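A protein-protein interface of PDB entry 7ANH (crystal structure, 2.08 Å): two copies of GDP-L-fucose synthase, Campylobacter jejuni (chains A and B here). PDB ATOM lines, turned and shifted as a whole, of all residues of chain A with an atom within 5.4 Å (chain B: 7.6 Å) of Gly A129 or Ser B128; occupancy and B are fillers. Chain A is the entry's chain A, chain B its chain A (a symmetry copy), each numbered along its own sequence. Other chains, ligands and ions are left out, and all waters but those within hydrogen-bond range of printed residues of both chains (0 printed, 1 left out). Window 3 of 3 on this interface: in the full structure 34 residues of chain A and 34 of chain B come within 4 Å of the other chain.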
ATOM      1  N   PRO A 114     -18.922  19.505 -12.665  1.00  0.00           N
ATOM      2  CA  PRO A 114     -17.759  19.833 -11.844  1.00  0.00           C
ATOM      3  C   PRO A 114     -17.888  21.249 -11.252  1.00  0.00           C
ATOM      4  O   PRO A 114     -18.509  22.143 -11.831  1.00  0.00           O
ATOM      5  CB  PRO A 114     -16.548  19.707 -12.825  1.00  0.00           C
ATOM      6  CG  PRO A 114     -17.038  18.951 -14.011  1.00  0.00           C
ATOM      7  CD  PRO A 114     -18.541  19.243 -14.071  1.00  0.00           C
ATOM      8  N   LYS A 115     -17.315  21.423 -10.080  1.00  0.00           N
ATOM      9  CA  LYS A 115     -17.326  22.676  -9.366  1.00  0.00           C
ATOM     10  C   LYS A 115     -16.531  23.774 -10.141  1.00  0.00           C
ATOM     11  O   LYS A 115     -16.913  24.920 -10.111  1.00  0.00           O
ATOM     12  CB  LYS A 115     -16.751  22.438  -7.973  1.00  0.00           C
ATOM     13  CG  LYS A 115     -16.726  23.665  -7.066  1.00  0.00           C
ATOM     14  CD  LYS A 115     -15.653  23.529  -5.988  1.00  0.00           C
ATOM     15  CE  LYS A 115     -15.761  24.644  -4.952  1.00  0.00           C
ATOM     16  NZ  LYS A 115     -15.407  24.173  -3.578  1.00  0.00           N
ATOM     17  N   GLN A 125     -19.555  18.660 -20.513  1.00  0.00           N
ATOM     18  CA  GLN A 125     -18.644  18.830 -19.427  1.00  0.00           C
ATOM     19  C   GLN A 125     -18.851  17.928 -18.209  1.00  0.00           C
ATOM     20  O   GLN A 125     -18.051  17.984 -17.269  1.00  0.00           O
ATOM     21  CB  GLN A 125     -18.609  20.328 -19.078  1.00  0.00           C
ATOM     22  CG  GLN A 125     -17.965  21.095 -20.239  1.00  0.00           C
ATOM     23  CD  GLN A 125     -18.157  22.554 -20.058  1.00  0.00           C
ATOM     24  OE1 GLN A 125     -18.960  23.220 -20.808  1.00  0.00           O
ATOM     25  NE2 GLN A 125     -17.466  23.098 -19.012  1.00  0.00           N
ATOM     26  N   LEU A 127     -18.327  15.221 -15.651  1.00  0.00           N
ATOM     27  CA  LEU A 127     -17.165  14.370 -15.226  1.00  0.00           C
ATOM     28  C   LEU A 127     -15.817  14.934 -15.666  1.00  0.00           C
ATOM     29  O   LEU A 127     -14.767  14.268 -15.508  1.00  0.00           O
ATOM     30  CB  LEU A 127     -17.292  12.925 -15.696  1.00  0.00           C
ATOM     31  CG  LEU A 127     -18.534  12.188 -15.183  1.00  0.00           C
ATOM     32  CD1 LEU A 127     -18.793  10.846 -15.856  1.00  0.00           C
ATOM     33  CD2 LEU A 127     -18.402  11.990 -13.689  1.00  0.00           C
ATOM     34  N   SER A 128     -15.789  16.196 -16.095  1.00  0.00           N
ATOM     35  CA  SER A 128     -14.540  16.730 -16.620  1.00  0.00           C
ATOM     36  C   SER A 128     -13.701  17.247 -15.459  1.00  0.00           C
ATOM     37  O   SER A 128     -12.589  17.706 -15.686  1.00  0.00           O
ATOM     38  CB  SER A 128     -14.773  17.807 -17.674  1.00  0.00           C
ATOM     39  OG  SER A 128     -15.574  18.845 -17.140  1.00  0.00           O
ATOM     40  N   GLY A 129     -14.215  17.134 -14.224  1.00  0.00           N
ATOM     41  CA  GLY A 129     -13.487  17.584 -13.051  1.00  0.00           C
ATOM     42  C   GLY A 129     -14.256  17.272 -11.799  1.00  0.00           C
ATOM     43  O   GLY A 129     -15.408  16.728 -11.848  1.00  0.00           O
ATOM     44  N   ASP A 130     -13.644  17.550 -10.665  1.00  0.00           N
ATOM     45  CA  ASP A 130     -14.152  17.064  -9.425  1.00  0.00           C
ATOM     46  C   ASP A 130     -15.408  17.786  -8.918  1.00  0.00           C
ATOM     47  O   ASP A 130     -15.666  18.927  -9.263  1.00  0.00           O
ATOM     48  CB  ASP A 130     -13.009  17.053  -8.361  1.00  0.00           C
ATOM     49  CG  ASP A 130     -13.315  16.138  -7.147  1.00  0.00           C
ATOM     50  OD1 ASP A 130     -14.375  15.456  -7.054  1.00  0.00           O
ATOM     51  OD2 ASP A 130     -12.478  16.139  -6.194  1.00  0.00           O
ATOM     52  N   LEU A 131     -16.196  17.108  -8.071  1.00  0.00           N
ATOM     53  CA  LEU A 131     -17.401  17.662  -7.525  1.00  0.00           C
ATOM     54  C   LEU A 131     -17.148  18.403  -6.226  1.00  0.00           C
ATOM     55  O   LEU A 131     -16.186  18.125  -5.540  1.00  0.00           O
ATOM     56  CB  LEU A 131     -18.425  16.542  -7.281  1.00  0.00           C
ATOM     57  CG  LEU A 131     -18.807  15.795  -8.573  1.00  0.00           C
ATOM     58  CD1 LEU A 131     -19.539  14.515  -8.215  1.00  0.00           C
ATOM     59  CD2 LEU A 131     -19.562  16.678  -9.577  1.00  0.00           C
ATOM     60  N   VAL B 112     -11.850   3.307 -11.528  1.00  0.00           N
ATOM     61  CA  VAL B 112     -12.432   4.569 -11.013  1.00  0.00           C
ATOM     62  C   VAL B 112     -11.711   5.841 -11.450  1.00  0.00           C
ATOM     63  O   VAL B 112     -12.216   6.979 -11.200  1.00  0.00           O
ATOM     64  CB  VAL B 112     -12.508   4.580  -9.477  1.00  0.00           C
ATOM     65  CG1 VAL B 112     -13.414   3.454  -8.928  1.00  0.00           C
ATOM     66  CG2 VAL B 112     -11.094   4.608  -8.872  1.00  0.00           C
ATOM     67  N   TYR B 113     -10.539   5.682 -12.095  1.00  0.00           N
ATOM     68  CA  TYR B 113      -9.714   6.864 -12.357  1.00  0.00           C
ATOM     69  C   TYR B 113      -9.928   7.423 -13.763  1.00  0.00           C
ATOM     70  O   TYR B 113     -10.310   6.646 -14.682  1.00  0.00           O
ATOM     71  CB  TYR B 113      -8.228   6.571 -12.115  1.00  0.00           C
ATOM     72  CG  TYR B 113      -7.927   6.394 -10.648  1.00  0.00           C
ATOM     73  CD1 TYR B 113      -8.084   7.456  -9.769  1.00  0.00           C
ATOM     74  CD2 TYR B 113      -7.512   5.134 -10.120  1.00  0.00           C
ATOM     75  CE1 TYR B 113      -7.882   7.290  -8.412  1.00  0.00           C
ATOM     76  CE2 TYR B 113      -7.302   4.942  -8.742  1.00  0.00           C
ATOM     77  CZ  TYR B 113      -7.457   5.989  -7.899  1.00  0.00           C
ATOM     78  OH  TYR B 113      -7.243   5.823  -6.557  1.00  0.00           O
ATOM     79  N   PRO B 114      -9.675   8.742 -13.933  1.00  0.00           N
ATOM     80  CA  PRO B 114      -9.852   9.321 -15.261  1.00  0.00           C
ATOM     81  C   PRO B 114      -8.901   8.661 -16.278  1.00  0.00           C
ATOM     82  O   PRO B 114      -7.806   8.203 -15.942  1.00  0.00           O
ATOM     83  CB  PRO B 114      -9.546  10.841 -15.062  1.00  0.00           C
ATOM     84  CG  PRO B 114      -9.600  11.097 -13.596  1.00  0.00           C
ATOM     85  CD  PRO B 114      -9.237   9.757 -12.948  1.00  0.00           C
ATOM     86  N   ASN B 116      -7.332  10.157 -18.754  1.00  0.00           N
ATOM     87  CA  ASN B 116      -6.166  10.972 -18.998  1.00  0.00           C
ATOM     88  C   ASN B 116      -5.513  11.484 -17.703  1.00  0.00           C
ATOM     89  O   ASN B 116      -4.888  12.574 -17.705  1.00  0.00           O
ATOM     90  CB  ASN B 116      -6.564  12.134 -19.903  1.00  0.00           C
ATOM     91  CG  ASN B 116      -7.213  11.658 -21.221  1.00  0.00           C
ATOM     92  OD1 ASN B 116      -6.774  10.671 -21.872  1.00  0.00           O
ATOM     93  ND2 ASN B 116      -8.276  12.365 -21.624  1.00  0.00           N
ATOM     94  N   ALA B 117      -5.632  10.716 -16.595  1.00  0.00           N
ATOM     95  CA  ALA B 117      -5.067  11.159 -15.285  1.00  0.00           C
ATOM     96  C   ALA B 117      -3.557  11.248 -15.371  1.00  0.00           C
ATOM     97  O   ALA B 117      -2.938  10.567 -16.189  1.00  0.00           O
ATOM     98  CB  ALA B 117      -5.444  10.193 -14.214  1.00  0.00           C
ATOM     99  N   THR B 118      -2.934  12.123 -14.621  1.00  0.00           N
ATOM    100  CA  THR B 118      -1.472  12.155 -14.686  1.00  0.00           C
ATOM    101  C   THR B 118      -0.863  11.038 -13.828  1.00  0.00           C
ATOM    102  O   THR B 118      -1.508  10.511 -12.907  1.00  0.00           O
ATOM    103  CB  THR B 118      -0.928  13.522 -14.372  1.00  0.00           C
ATOM    104  OG1 THR B 118      -1.487  13.951 -13.143  1.00  0.00           O
ATOM    105  CG2 THR B 118      -1.331  14.506 -15.497  1.00  0.00           C
ATOM    106  N   THR B 121      -0.738   8.017 -10.469  1.00  0.00           N
ATOM    107  CA  THR B 121      -2.126   8.345 -10.199  1.00  0.00           C
ATOM    108  C   THR B 121      -2.471   8.058  -8.752  1.00  0.00           C
ATOM    109  O   THR B 121      -2.700   6.896  -8.341  1.00  0.00           O
ATOM    110  CB  THR B 121      -3.050   7.627 -11.206  1.00  0.00           C
ATOM    111  OG1 THR B 121      -2.489   7.779 -12.544  1.00  0.00           O
ATOM    112  CG2 THR B 121      -4.469   8.191 -11.122  1.00  0.00           C
ATOM    113  N   SER B 122      -2.516   9.116  -7.951  1.00  0.00           N
ATOM    114  CA  SER B 122      -2.879   8.918  -6.550  1.00  0.00           C
ATOM    115  C   SER B 122      -4.408   8.891  -6.392  1.00  0.00           C
ATOM    116  O   SER B 122      -5.128   9.305  -7.294  1.00  0.00           O
ATOM    117  CB  SER B 122      -2.184   9.945  -5.646  1.00  0.00           C
ATOM    118  OG  SER B 122      -2.989  11.030  -5.384  1.00  0.00           O
ATOM    119  N   GLU B 124      -6.045  10.862  -4.821  1.00  0.00           N
ATOM    120  CA  GLU B 124      -6.530  12.251  -4.957  1.00  0.00           C
ATOM    121  C   GLU B 124      -6.921  12.658  -6.388  1.00  0.00           C
ATOM    122  O   GLU B 124      -7.604  13.598  -6.600  1.00  0.00           O
ATOM    123  CB  GLU B 124      -5.575  13.277  -4.334  1.00  0.00           C
ATOM    124  CG  GLU B 124      -5.284  13.054  -2.842  1.00  0.00           C
ATOM    125  CD  GLU B 124      -6.528  12.895  -1.937  1.00  0.00           C
ATOM    126  OE1 GLU B 124      -7.636  13.430  -2.168  1.00  0.00           O
ATOM    127  OE2 GLU B 124      -6.401  12.256  -0.907  1.00  0.00           O
ATOM    128  N   GLN B 125      -6.545  11.883  -7.371  1.00  0.00           N
ATOM    129  CA  GLN B 125      -6.976  12.155  -8.705  1.00  0.00           C
ATOM    130  C   GLN B 125      -8.345  11.607  -9.111  1.00  0.00           C
ATOM    131  O   GLN B 125      -8.798  11.871 -10.230  1.00  0.00           O
ATOM    132  CB  GLN B 125      -5.843  11.732  -9.656  1.00  0.00           C
ATOM    133  CG  GLN B 125      -4.643  12.661  -9.446  1.00  0.00           C
ATOM    134  CD  GLN B 125      -3.449  12.123 -10.144  1.00  0.00           C
ATOM    135  OE1 GLN B 125      -2.460  11.628  -9.490  1.00  0.00           O
ATOM    136  NE2 GLN B 125      -3.523  12.146 -11.508  1.00  0.00           N
ATOM    137  N   MET B 126      -9.039  10.910  -8.204  1.00  0.00           N
ATOM    138  CA  MET B 126     -10.354  10.434  -8.518  1.00  0.00           C
ATOM    139  C   MET B 126     -11.279  11.619  -8.937  1.00  0.00           C
ATOM    140  O   MET B 126     -11.311  12.635  -8.252  1.00  0.00           O
ATOM    141  CB  MET B 126     -10.988   9.636  -7.390  1.00  0.00           C
ATOM    142  CG  MET B 126     -12.117   8.778  -7.950  1.00  0.00           C
ATOM    143  SD  MET B 126     -12.838   7.591  -6.837  1.00  0.00           S
ATOM    144  CE  MET B 126     -13.341   8.646  -5.443  1.00  0.00           C
ATOM    145  N   LEU B 127     -11.980  11.452 -10.064  1.00  0.00           N
ATOM    146  CA  LEU B 127     -12.990  12.443 -10.567  1.00  0.00           C
ATOM    147  C   LEU B 127     -12.356  13.703 -11.150  1.00  0.00           C
ATOM    148  O   LEU B 127     -13.069  14.679 -11.482  1.00  0.00           O
ATOM    149  CB  LEU B 127     -14.013  12.830  -9.505  1.00  0.00           C
ATOM    150  CG  LEU B 127     -14.839  11.664  -8.952  1.00  0.00           C
ATOM    151  CD1 LEU B 127     -15.666  12.009  -7.718  1.00  0.00           C
ATOM    152  CD2 LEU B 127     -15.748  11.148 -10.045  1.00  0.00           C
ATOM    153  N   SER B 128     -11.048  13.669 -11.409  1.00  0.00           N
ATOM    154  CA  SER B 128     -10.394  14.887 -11.867  1.00  0.00           C
ATOM    155  C   SER B 128     -10.555  14.994 -13.377  1.00  0.00           C
ATOM    156  O   SER B 128     -10.102  15.973 -13.956  1.00  0.00           O
ATOM    157  CB  SER B 128      -8.928  14.943 -11.447  1.00  0.00           C
ATOM    158  OG  SER B 128      -8.242  13.799 -11.922  1.00  0.00           O
ATOM    159  N   GLY B 129     -11.229  14.014 -13.999  1.00  0.00           N
ATOM    160  CA  GLY B 129     -11.447  14.031 -15.434  1.00  0.00           C
ATOM    161  C   GLY B 129     -12.290  12.861 -15.856  1.00  0.00           C
ATOM    162  O   GLY B 129     -12.679  11.988 -15.012  1.00  0.00           O
ATOM    163  N   ASP B 130     -12.634  12.829 -17.127  1.00  0.00           N
ATOM    164  CA  ASP B 130     -13.636  11.927 -17.590  1.00  0.00           C
ATOM    165  C   ASP B 130     -13.188  10.461 -17.679  1.00  0.00           C
ATOM    166  O   ASP B 130     -12.012  10.165 -17.809  1.00  0.00           O
ATOM    167  CB  ASP B 130     -14.226  12.447 -18.938  1.00  0.00           C
ATOM    168  CG  ASP B 130     -15.599  11.816 -19.286  1.00  0.00           C
ATOM    169  OD1 ASP B 130     -16.183  10.988 -18.532  1.00  0.00           O
ATOM    170  OD2 ASP B 130     -16.108  12.118 -20.408  1.00  0.00           O
ATOM    171  N   LEU B 131     -14.150   9.529 -17.625  1.00  0.00           N
ATOM    172  CA  LEU B 131     -13.870   8.124 -17.693  1.00  0.00           C
ATOM    173  C   LEU B 131     -13.873   7.614 -19.121  1.00  0.00           C
ATOM    174  O   LEU B 131     -14.501   8.199 -19.980  1.00  0.00           O
ATOM    175  CB  LEU B 131     -14.911   7.345 -16.873  1.00  0.00           C
ATOM    176  CG  LEU B 131     -14.910   7.741 -15.384  1.00  0.00           C
ATOM    177  CD1 LEU B 131     -16.162   7.197 -14.719  1.00  0.00           C
ATOM    178  CD2 LEU B 131     -13.611   7.359 -14.661  1.00  0.00           C
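The backbone NH of Asp B130 sits at hydrogen-bond distance from the backbone carbonyl oxygen of Leu A127, 3.0 Å away. The backbone carbonyl oxygen (O) of Leu B127 sits at hydrogen-bond distance from the backbone NH (N) of Asp A130 (3.0 Å). The backbone carbonyl oxygen (O) of Gly B129 sits close to the backbone carbonyl oxygen (O) of Leu A127, at 3.1 Å. O of Ser B128 sits close to O of Ser A128. O of Gly A129 lies close to O of Leu B127 (3.1 Å).
The backbone NH (N) of Lys A115 lies within hydrogen-bond range of the backbone carbonyl oxygen (O) of Asp A130 (3.1 Å). The side-chain hydroxyl (OG) of Ser A128 sits at hydrogen-bond distance from the backbone carbonyl oxygen (O) of Gln A125, at 2.6 Å. O of Gln B125 sits at hydrogen-bond distance from OG of Ser B128, at 2.6 Å.
CA of Gly B129 touches O of Ser A128, at 3.9 Å. Ser B128 touches Gly A129 (O to CA, 3.9 Å).
Lys A115 touches none of the printed residues of chain B. Of the printed residues of chain B, Leu A127 touches Gly B129 (2.9 Å) and Asp B130 (3.0 Å). Gly A129 touches two residues of chain B. Of the printed residues of chain B, Asp A130 touches Leu B127. Ala B117 touches none of the printed residues of chain A. Of chain A, only Ser A128 (3.5 Å) and Gly A129 (3.9 Å) come within 4 Å of Ser B128. Printed residues of chain A within 4 Å of Gly B129: Leu A127 and Ser A128. Printed residues of chain A within 4 Å of Asp B130: Leu A127. The nearest residue of chain A that does not touch Ser B128 is Asp A130 (4.4 Å).
Hydrophobic or aromatic side chains of chain B within 4 Å of the printed part of chain A: Leu B127. Hydrophobic or aromatic side chains of chain A that line the printed part of chain B: Leu A127. Among the printed residues, no Asp or Glu carboxylate lies within 4 Å of a Lys or Arg side-chain nitrogen of the other chain.
Leu A127 touches Gly B129, and with the chains exchanged Gly A129 touches Leu B127. Leu A127 touches Asp B130, and with the chains exchanged Asp A130 touches Leu B127. Ser B128 touches its own counterpart, Ser A128. Ser A128 touches Gly B129, and with the chains exchanged Gly A129 touches Ser B128. Positions printed for both chains: 114, 125, 127, 128, 129, 130 and 131. Of the 7 pairs that touch across the chains among the printed residues, 7 have their exchanged pair printed and touching as well.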
